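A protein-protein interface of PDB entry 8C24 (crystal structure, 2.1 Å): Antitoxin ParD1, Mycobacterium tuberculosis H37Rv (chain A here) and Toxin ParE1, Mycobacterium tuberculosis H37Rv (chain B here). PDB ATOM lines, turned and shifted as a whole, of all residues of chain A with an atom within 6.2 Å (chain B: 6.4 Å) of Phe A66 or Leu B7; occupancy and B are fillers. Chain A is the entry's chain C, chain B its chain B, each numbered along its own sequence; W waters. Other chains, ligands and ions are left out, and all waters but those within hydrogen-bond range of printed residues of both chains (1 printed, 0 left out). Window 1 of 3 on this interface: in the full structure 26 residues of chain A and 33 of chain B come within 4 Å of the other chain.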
ATOM      1  N   SER A  62      -3.556  11.311 -15.984  1.00  0.00           N
ATOM      2  CA  SER A  62      -4.015   9.958 -16.271  1.00  0.00           C
ATOM      3  C   SER A  62      -3.561   8.991 -15.183  1.00  0.00           C
ATOM      4  O   SER A  62      -2.441   9.081 -14.664  1.00  0.00           O
ATOM      5  CB  SER A  62      -3.498   9.475 -17.629  1.00  0.00           C
ATOM      6  OG  SER A  62      -4.464   9.755 -18.632  1.00  0.00           O
ATOM      7  N   SER A  63      -4.446   8.062 -14.844  1.00  0.00           N
ATOM      8  CA  SER A  63      -4.140   7.028 -13.857  1.00  0.00           C
ATOM      9  C   SER A  63      -3.246   5.957 -14.482  1.00  0.00           C
ATOM     10  O   SER A  63      -3.437   5.588 -15.639  1.00  0.00           O
ATOM     11  CB  SER A  63      -5.438   6.401 -13.353  1.00  0.00           C
ATOM     12  OG  SER A  63      -6.233   7.325 -12.616  1.00  0.00           O
ATOM     13  N   THR A  64      -2.267   5.459 -13.722  1.00  0.00           N
ATOM     14  CA  THR A  64      -1.334   4.456 -14.230  1.00  0.00           C
ATOM     15  C   THR A  64      -1.329   3.236 -13.326  1.00  0.00           C
ATOM     16  O   THR A  64      -1.803   3.303 -12.181  1.00  0.00           O
ATOM     17  CB  THR A  64       0.107   4.987 -14.331  1.00  0.00           C
ATOM     18  OG1 THR A  64       0.692   5.066 -13.024  1.00  0.00           O
ATOM     19  CG2 THR A  64       0.160   6.351 -15.016  1.00  0.00           C
ATOM     20  N   PRO A  65      -0.792   2.104 -13.795  1.00  0.00           N
ATOM     21  CA  PRO A  65      -0.556   0.982 -12.878  1.00  0.00           C
ATOM     22  C   PRO A  65       0.432   1.390 -11.798  1.00  0.00           C
ATOM     23  O   PRO A  65       1.155   2.383 -11.919  1.00  0.00           O
ATOM     24  CB  PRO A  65       0.012  -0.120 -13.784  1.00  0.00           C
ATOM     25  CG  PRO A  65      -0.441   0.264 -15.203  1.00  0.00           C
ATOM     26  CD  PRO A  65      -0.447   1.766 -15.197  1.00  0.00           C
ATOM     27  N   PHE A  66       0.436   0.623 -10.709  1.00  0.00           N
ATOM     28  CA  PHE A  66       1.243   0.950  -9.544  1.00  0.00           C
ATOM     29  C   PHE A  66       1.792  -0.344  -8.967  1.00  0.00           C
ATOM     30  O   PHE A  66       1.037  -1.301  -8.776  1.00  0.00           O
ATOM     31  CB  PHE A  66       0.417   1.692  -8.493  1.00  0.00           C
ATOM     32  CG  PHE A  66       1.216   2.202  -7.323  1.00  0.00           C
ATOM     33  CD1 PHE A  66       1.888   3.410  -7.403  1.00  0.00           C
ATOM     34  CD2 PHE A  66       1.275   1.482  -6.136  1.00  0.00           C
ATOM     35  CE1 PHE A  66       2.607   3.892  -6.320  1.00  0.00           C
ATOM     36  CE2 PHE A  66       2.001   1.955  -5.045  1.00  0.00           C
ATOM     37  CZ  PHE A  66       2.667   3.160  -5.135  1.00  0.00           C
ATOM     38  N   ASP A  67       3.098  -0.355  -8.688  1.00  0.00           N
ATOM     39  CA  ASP A  67       3.857  -1.545  -8.298  1.00  0.00           C
ATOM     40  C   ASP A  67       4.168  -1.420  -6.808  1.00  0.00           C
ATOM     41  O   ASP A  67       5.152  -0.792  -6.414  1.00  0.00           O
ATOM     42  CB  ASP A  67       5.128  -1.648  -9.178  1.00  0.00           C
ATOM     43  CG  ASP A  67       6.124  -2.714  -8.708  1.00  0.00           C
ATOM     44  OD1 ASP A  67       5.873  -3.433  -7.707  1.00  0.00           O
ATOM     45  OD2 ASP A  67       7.186  -2.822  -9.367  1.00  0.00           O
ATOM     46  N   PHE A  68       3.320  -2.035  -5.976  1.00  0.00           N
ATOM     47  CA  PHE A  68       3.490  -1.918  -4.529  1.00  0.00           C
ATOM     48  C   PHE A  68       4.814  -2.495  -4.061  1.00  0.00           C
ATOM     49  O   PHE A  68       5.488  -1.899  -3.208  1.00  0.00           O
ATOM     50  CB  PHE A  68       2.337  -2.603  -3.801  1.00  0.00           C
ATOM     51  CG  PHE A  68       1.262  -1.654  -3.378  1.00  0.00           C
ATOM     52  CD1 PHE A  68       1.394  -0.919  -2.214  1.00  0.00           C
ATOM     53  CD2 PHE A  68       0.133  -1.480  -4.162  1.00  0.00           C
ATOM     54  CE1 PHE A  68       0.399  -0.019  -1.825  1.00  0.00           C
ATOM     55  CE2 PHE A  68      -0.860  -0.590  -3.786  1.00  0.00           C
ATOM     56  CZ  PHE A  68      -0.720   0.141  -2.611  1.00  0.00           C
ATOM     57  N   PHE A  71       7.493  -0.057  -5.048  1.00  0.00           N
ATOM     58  CA  PHE A  71       7.353   1.150  -4.238  1.00  0.00           C
ATOM     59  C   PHE A  71       7.795   0.900  -2.803  1.00  0.00           C
ATOM     60  O   PHE A  71       8.565   1.685  -2.234  1.00  0.00           O
ATOM     61  CB  PHE A  71       5.911   1.649  -4.288  1.00  0.00           C
ATOM     62  CG  PHE A  71       5.550   2.593  -3.166  1.00  0.00           C
ATOM     63  CD1 PHE A  71       5.976   3.913  -3.187  1.00  0.00           C
ATOM     64  CD2 PHE A  71       4.779   2.157  -2.096  1.00  0.00           C
ATOM     65  CE1 PHE A  71       5.645   4.787  -2.158  1.00  0.00           C
ATOM     66  CE2 PHE A  71       4.434   3.026  -1.061  1.00  0.00           C
ATOM     67  CZ  PHE A  71       4.868   4.349  -1.096  1.00  0.00           C
ATOM     68  N   ARG A  74      11.655   0.323  -2.742  1.00  0.00           N
ATOM     69  CA  ARG A  74      12.391   1.580  -2.864  1.00  0.00           C
ATOM     70  C   ARG A  74      12.345   2.389  -1.579  1.00  0.00           C
ATOM     71  O   ARG A  74      13.362   2.949  -1.150  1.00  0.00           O
ATOM     72  CB  ARG A  74      11.829   2.430  -4.009  1.00  0.00           C
ATOM     73  CG  ARG A  74      12.059   3.935  -3.780  1.00  0.00           C
ATOM     74  CD  ARG A  74      11.773   4.801  -4.997  1.00  0.00           C
ATOM     75  NE  ARG A  74      10.365   4.799  -5.386  1.00  0.00           N
ATOM     76  CZ  ARG A  74       9.461   5.656  -4.916  1.00  0.00           C
ATOM     77  NH1 ARG A  74       9.823   6.574  -4.028  1.00  0.00           N
ATOM     78  NH2 ARG A  74       8.199   5.593  -5.328  1.00  0.00           N
ATOM     79  N   ARG B   4      -6.020  -6.189 -12.076  1.00  0.00           N
ATOM     80  CA  ARG B   4      -5.228  -4.966 -12.339  1.00  0.00           C
ATOM     81  C   ARG B   4      -6.042  -3.752 -11.908  1.00  0.00           C
ATOM     82  O   ARG B   4      -7.266  -3.819 -11.876  1.00  0.00           O
ATOM     83  CB  ARG B   4      -4.796  -4.843 -13.800  1.00  0.00           C
ATOM     84  CG  ARG B   4      -3.302  -4.612 -13.980  1.00  0.00           C
ATOM     85  CD  ARG B   4      -2.664  -3.484 -13.191  1.00  0.00           C
ATOM     86  NE  ARG B   4      -1.752  -3.921 -12.146  1.00  0.00           N
ATOM     87  CZ  ARG B   4      -1.286  -3.166 -11.155  1.00  0.00           C
ATOM     88  NH1 ARG B   4      -0.449  -3.687 -10.278  1.00  0.00           N
ATOM     89  NH2 ARG B   4      -1.642  -1.903 -11.031  1.00  0.00           N
ATOM     90  N   TYR B   5      -5.335  -2.697 -11.552  1.00  0.00           N
ATOM     91  CA  TYR B   5      -5.968  -1.458 -11.134  1.00  0.00           C
ATOM     92  C   TYR B   5      -5.061  -0.307 -11.530  1.00  0.00           C
ATOM     93  O   TYR B   5      -3.857  -0.486 -11.735  1.00  0.00           O
ATOM     94  CB  TYR B   5      -6.219  -1.423  -9.616  1.00  0.00           C
ATOM     95  CG  TYR B   5      -5.000  -1.764  -8.778  1.00  0.00           C
ATOM     96  CD1 TYR B   5      -4.077  -0.789  -8.419  1.00  0.00           C
ATOM     97  CD2 TYR B   5      -4.780  -3.063  -8.333  1.00  0.00           C
ATOM     98  CE1 TYR B   5      -2.957  -1.107  -7.654  1.00  0.00           C
ATOM     99  CE2 TYR B   5      -3.676  -3.382  -7.563  1.00  0.00           C
ATOM    100  CZ  TYR B   5      -2.773  -2.400  -7.225  1.00  0.00           C
ATOM    101  OH  TYR B   5      -1.678  -2.729  -6.457  1.00  0.00           O
ATOM    102  N   LEU B   6      -5.644   0.887 -11.607  1.00  0.00           N
ATOM    103  CA  LEU B   6      -4.885   2.097 -11.873  1.00  0.00           C
ATOM    104  C   LEU B   6      -5.008   3.027 -10.680  1.00  0.00           C
ATOM    105  O   LEU B   6      -6.062   3.087 -10.040  1.00  0.00           O
ATOM    106  CB  LEU B   6      -5.380   2.792 -13.156  1.00  0.00           C
ATOM    107  CG  LEU B   6      -5.627   1.889 -14.366  1.00  0.00           C
ATOM    108  CD1 LEU B   6      -6.381   2.614 -15.456  1.00  0.00           C
ATOM    109  CD2 LEU B   6      -4.304   1.352 -14.895  1.00  0.00           C
ATOM    110  N   LEU B   7      -3.926   3.738 -10.376  1.00  0.00           N
ATOM    111  CA  LEU B   7      -3.931   4.808  -9.386  1.00  0.00           C
ATOM    112  C   LEU B   7      -3.706   6.156 -10.067  1.00  0.00           C
ATOM    113  O   LEU B   7      -2.848   6.273 -10.947  1.00  0.00           O
ATOM    114  CB  LEU B   7      -2.851   4.592  -8.337  1.00  0.00           C
ATOM    115  CG  LEU B   7      -2.837   3.226  -7.633  1.00  0.00           C
ATOM    116  CD1 LEU B   7      -1.958   3.298  -6.409  1.00  0.00           C
ATOM    117  CD2 LEU B   7      -4.241   2.784  -7.269  1.00  0.00           C
ATOM    118  N   SER B   8      -4.468   7.177  -9.652  1.00  0.00           N
ATOM    119  CA  SER B   8      -4.255   8.520 -10.165  1.00  0.00           C
ATOM    120  C   SER B   8      -2.925   9.038  -9.638  1.00  0.00           C
ATOM    121  O   SER B   8      -2.435   8.554  -8.612  1.00  0.00           O
ATOM    122  CB  SER B   8      -5.388   9.456  -9.734  1.00  0.00           C
ATOM    123  OG  SER B   8      -5.265   9.763  -8.353  1.00  0.00           O
ATOM    124  N   PRO B   9      -2.296   9.995 -10.342  1.00  0.00           N
ATOM    125  CA  PRO B   9      -1.094  10.634  -9.773  1.00  0.00           C
ATOM    126  C   PRO B   9      -1.332  11.156  -8.365  1.00  0.00           C
ATOM    127  O   PRO B   9      -0.484  10.972  -7.483  1.00  0.00           O
ATOM    128  CB  PRO B   9      -0.790  11.764 -10.762  1.00  0.00           C
ATOM    129  CG  PRO B   9      -1.374  11.300 -12.076  1.00  0.00           C
ATOM    130  CD  PRO B   9      -2.566  10.433 -11.725  1.00  0.00           C
ATOM    131  N   ALA B  10      -2.483  11.788  -8.123  1.00  0.00           N
ATOM    132  CA  ALA B  10      -2.818  12.234  -6.775  1.00  0.00           C
ATOM    133  C   ALA B  10      -2.734  11.082  -5.769  1.00  0.00           C
ATOM    134  O   ALA B  10      -2.092  11.204  -4.721  1.00  0.00           O
ATOM    135  CB  ALA B  10      -4.216  12.854  -6.768  1.00  0.00           C
ATOM    136  N   ALA B  11      -3.367   9.947  -6.090  1.00  0.00           N
ATOM    137  CA  ALA B  11      -3.406   8.813  -5.163  1.00  0.00           C
ATOM    138  C   ALA B  11      -2.015   8.228  -4.912  1.00  0.00           C
ATOM    139  O   ALA B  11      -1.680   7.873  -3.772  1.00  0.00           O
ATOM    140  CB  ALA B  11      -4.351   7.737  -5.705  1.00  0.00           C
ATOM    141  N   GLN B  12      -1.196   8.090  -5.961  1.00  0.00           N
ATOM    142  CA  GLN B  12       0.164   7.596  -5.761  1.00  0.00           C
ATOM    143  C   GLN B  12       0.946   8.514  -4.830  1.00  0.00           C
ATOM    144  O   GLN B  12       1.611   8.052  -3.893  1.00  0.00           O
ATOM    145  CB  GLN B  12       0.881   7.457  -7.110  1.00  0.00           C
ATOM    146  CG  GLN B  12       0.103   6.649  -8.131  1.00  0.00           C
ATOM    147  CD  GLN B  12       0.946   6.288  -9.340  1.00  0.00           C
ATOM    148  OE1 GLN B  12       2.163   6.470  -9.330  1.00  0.00           O
ATOM    149  NE2 GLN B  12       0.303   5.792 -10.391  1.00  0.00           N
ATOM    150  N   ALA B  13       0.868   9.823  -5.067  1.00  0.00           N
ATOM    151  CA  ALA B  13       1.551  10.776  -4.196  1.00  0.00           C
ATOM    152  C   ALA B  13       1.077  10.654  -2.747  1.00  0.00           C
ATOM    153  O   ALA B  13       1.859  10.860  -1.807  1.00  0.00           O
ATOM    154  CB  ALA B  13       1.320  12.199  -4.710  1.00  0.00           C
ATOM    155  N   LEU B  15      -0.146   7.866  -1.246  1.00  0.00           N
ATOM    156  CA  LEU B  15       0.461   6.656  -0.700  1.00  0.00           C
ATOM    157  C   LEU B  15       1.863   6.947  -0.192  1.00  0.00           C
ATOM    158  O   LEU B  15       2.234   6.528   0.909  1.00  0.00           O
ATOM    159  CB  LEU B  15       0.491   5.543  -1.750  1.00  0.00           C
ATOM    160  CG  LEU B  15      -0.893   5.043  -2.149  1.00  0.00           C
ATOM    161  CD1 LEU B  15      -0.796   3.805  -3.007  1.00  0.00           C
ATOM    162  CD2 LEU B  15      -1.770   4.806  -0.919  1.00  0.00           C
ATOM    163  N   GLU B  16       2.634   7.712  -0.959  1.00  0.00           N
ATOM    164  CA  GLU B  16       3.988   8.044  -0.543  1.00  0.00           C
ATOM    165  C   GLU B  16       3.983   8.914   0.710  1.00  0.00           C
ATOM    166  O   GLU B  16       4.799   8.710   1.615  1.00  0.00           O
ATOM    167  CB  GLU B  16       4.739   8.727  -1.693  1.00  0.00           C
ATOM    168  CG  GLU B  16       6.257   8.750  -1.482  1.00  0.00           C
ATOM    169  CD  GLU B  16       7.072   8.742  -2.769  1.00  0.00           C
ATOM    170  OE1 GLU B  16       7.777   9.740  -3.014  1.00  0.00           O
ATOM    171  OE2 GLU B  16       7.026   7.746  -3.528  1.00  0.00           O
ATOM    172  N   LEU B  35       0.884   0.257   4.499  1.00  0.00           N
ATOM    173  CA  LEU B  35       0.686   0.361   3.056  1.00  0.00           C
ATOM    174  C   LEU B  35       0.198  -0.967   2.491  1.00  0.00           C
ATOM    175  O   LEU B  35      -0.636  -0.992   1.570  1.00  0.00           O
ATOM    176  CB  LEU B  35       1.968   0.840   2.365  1.00  0.00           C
ATOM    177  CG  LEU B  35       2.067   2.343   2.039  1.00  0.00           C
ATOM    178  CD1 LEU B  35       0.922   2.805   1.139  1.00  0.00           C
ATOM    179  CD2 LEU B  35       2.092   3.182   3.297  1.00  0.00           C
ATOM    180  N   ILE B  42      -7.220  -2.273  -1.850  1.00  0.00           N
ATOM    181  CA  ILE B  42      -7.182  -2.022  -3.297  1.00  0.00           C
ATOM    182  C   ILE B  42      -7.369  -3.326  -4.066  1.00  0.00           C
ATOM    183  O   ILE B  42      -8.167  -3.399  -5.008  1.00  0.00           O
ATOM    184  CB  ILE B  42      -5.877  -1.301  -3.688  1.00  0.00           C
ATOM    185  CG1 ILE B  42      -5.896   0.129  -3.119  1.00  0.00           C
ATOM    186  CG2 ILE B  42      -5.677  -1.281  -5.240  1.00  0.00           C
ATOM    187  CD1 ILE B  42      -4.538   0.832  -3.177  1.00  0.00           C
ATOM    188  N   ILE B  82     -10.511  -1.092 -12.063  1.00  0.00           N
ATOM    189  CA  ILE B  82     -10.798   0.038 -11.183  1.00  0.00           C
ATOM    190  C   ILE B  82      -9.713   1.100 -11.335  1.00  0.00           C
ATOM    191  O   ILE B  82      -8.534   0.812 -11.565  1.00  0.00           O
ATOM    192  CB  ILE B  82     -10.963  -0.392  -9.705  1.00  0.00           C
ATOM    193  CG1 ILE B  82      -9.617  -0.772  -9.071  1.00  0.00           C
ATOM    194  CG2 ILE B  82     -12.008  -1.505  -9.566  1.00  0.00           C
ATOM    195  CD1 ILE B  82      -9.718  -1.060  -7.580  1.00  0.00           C
ATOM    196  N   ASP B  83     -10.135   2.352 -11.198  1.00  0.00           N
ATOM    197  CA  ASP B  83      -9.280   3.538 -11.275  1.00  0.00           C
ATOM    198  C   ASP B  83      -9.435   4.263  -9.933  1.00  0.00           C
ATOM    199  O   ASP B  83     -10.461   4.903  -9.675  1.00  0.00           O
ATOM    200  CB  ASP B  83      -9.691   4.407 -12.484  1.00  0.00           C
ATOM    201  CG  ASP B  83      -8.984   5.774 -12.534  1.00  0.00           C
ATOM    202  OD1 ASP B  83      -8.036   6.024 -11.758  1.00  0.00           O
ATOM    203  OD2 ASP B  83      -9.390   6.611 -13.373  1.00  0.00           O
ATOM    204  N   VAL B  84      -8.423   4.158  -9.074  1.00  0.00           N
ATOM    205  CA  VAL B  84      -8.472   4.767  -7.752  1.00  0.00           C
ATOM    206  C   VAL B  84      -8.056   6.232  -7.890  1.00  0.00           C
ATOM    207  O   VAL B  84      -6.876   6.533  -8.091  1.00  0.00           O
ATOM    208  CB  VAL B  84      -7.580   4.012  -6.759  1.00  0.00           C
ATOM    209  CG1 VAL B  84      -7.568   4.693  -5.424  1.00  0.00           C
ATOM    210  CG2 VAL B  84      -8.046   2.555  -6.614  1.00  0.00           C
ATOM    211  N   VAL B  85      -9.032   7.149  -7.776  1.00  0.00           N
ATOM    212  CA  VAL B  85      -8.785   8.579  -8.004  1.00  0.00           C
ATOM    213  C   VAL B  85      -8.251   9.263  -6.745  1.00  0.00           C
ATOM    214  O   VAL B  85      -7.378  10.133  -6.826  1.00  0.00           O
ATOM    215  CB  VAL B  85     -10.070   9.257  -8.517  1.00  0.00           C
ATOM    216  CG1 VAL B  85      -9.824  10.748  -8.859  1.00  0.00           C
ATOM    217  CG2 VAL B  85     -10.632   8.497  -9.712  1.00  0.00           C
HETATM  218  O   HOH W   1       1.275  -3.071  -6.778  1.00  0.00           O
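Among the printed residues, pairs that only touch across the chains: Phe A68 with Tyr B5, Ser A62 with Pro B9, Ser A63 with Leu B7, Thr A64 with Leu B6, Phe A66 with Leu B7, Phe A71 with Glu B16, Pro A65 with Arg B4, Phe A66 with Gln B12, Ser A63 with Leu B6, Phe A68 with Leu B35, Phe A68 with Leu B15, Pro A65 with Leu B6, Pro A65 with Tyr B5, Pro A65 with Gln B12, Phe A66 with Tyr B5, Phe A68 with Ile B42, Phe A66 with Leu B15, Phe A71 with Leu B35 and Phe A71 with Leu B15.
Phe A66 touches just these residues of chain B: Arg B4 (3.2 Å), Tyr B5 (3.8 Å), Leu B7 (3.5 Å), Gln B12 (3.6 Å) and Leu B15 (3.9 Å). Leu B7 touches just these residues of chain A: Ser A63 (3.3 Å), Thr A64 (2.8 Å) and Phe A66 (3.5 Å). Printed residues of chain A within 4 Å of Glu B16: Phe A71 and Arg A74. Of the printed residues of chain B, Phe A71 touches Leu B15, Glu B16 and Leu B35. Printed residues of chain A within 4 Å of Ile B42: Phe A68 (3.9 Å). Of the printed residues of chain A, Ser B8 touches Ser A63 (3.4 Å). Ile B82 touches none of the printed residues of chain A. The nearest residue of chain A that does not touch Leu B7 is Ser A62 (4.7 Å). The nearest printed residue of chain A that does not touch Leu B6 is Phe A66 (5.6 Å).
Of the 18 printed residues of chain B, 12 touch a printed residue of chain A. Hydrophobic or aromatic side chains of chain B within 4 Å of the printed part of chain A: Tyr B5, Leu B6, Leu B7, Pro B9, Leu B15, Leu B35 and Ile B42. Hydrophobic or aromatic side chains of chain A that line the printed part of chain B: Pro A65, Phe A66, Phe A68 and Phe A71. Along chain A the printed residues that touch a printed residue of chain B span positions 62 to 74. Among the printed residues, Asp or Glu carboxylates within 4 Å of a Lys or Arg side-chain nitrogen of the other chain: Arg A74 with Glu B16.
OG of Ser A63 lies close to OD2 of Asp B83, 3.3 Å away. The side-chain hydroxyl (OG1) of Thr A64 is in hydrogen-bond range of the side-chain amide nitrogen (NE2) of Gln B12 (2.8 Å). N of Ser B8 lies close to OG of Ser A63 (3.5 Å). The backbone NH (N) of Leu B7 is in hydrogen-bond range of the backbone carbonyl oxygen (O) of Thr A64 (2.8 Å). NH2 of Arg A74 is in salt-bridge range of OE2 of Glu B16, 3.0 Å away. The guanidinium group of Arg B4 lies within hydrogen-bond range of the backbone carbonyl oxygen of Phe A66.
The backbone carbonyl oxygen (O) of Leu B7 sits at hydrogen-bond distance from the side-chain amide nitrogen (NE2) of Gln B12, at 3.2 Å. The side-chain hydroxyl (OG) of Ser B8 lies close to the backbone NH (N) of Ala B10, at 3.4 Å. OG of Ser B8 is in hydrogen-bond range of O of Val B85, at 2.6 Å. N of Leu B6 is in hydrogen-bond range of O of Ile B82, 2.9 Å away. O of Leu B6 lies within hydrogen-bond range of N of Val B84, 2.8 Å away. The backbone NH of Ser B8 lies within hydrogen-bond range of the backbone carbonyl oxygen of Val B84 (2.9 Å).
Water W1 lies within hydrogen-bond range of the backbone NH of Phe A68 (2.4 Å), the backbone carbonyl oxygen of Phe A66 (2.7 Å) and the side-chain hydroxyl of Tyr B5 (3.0 Å).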
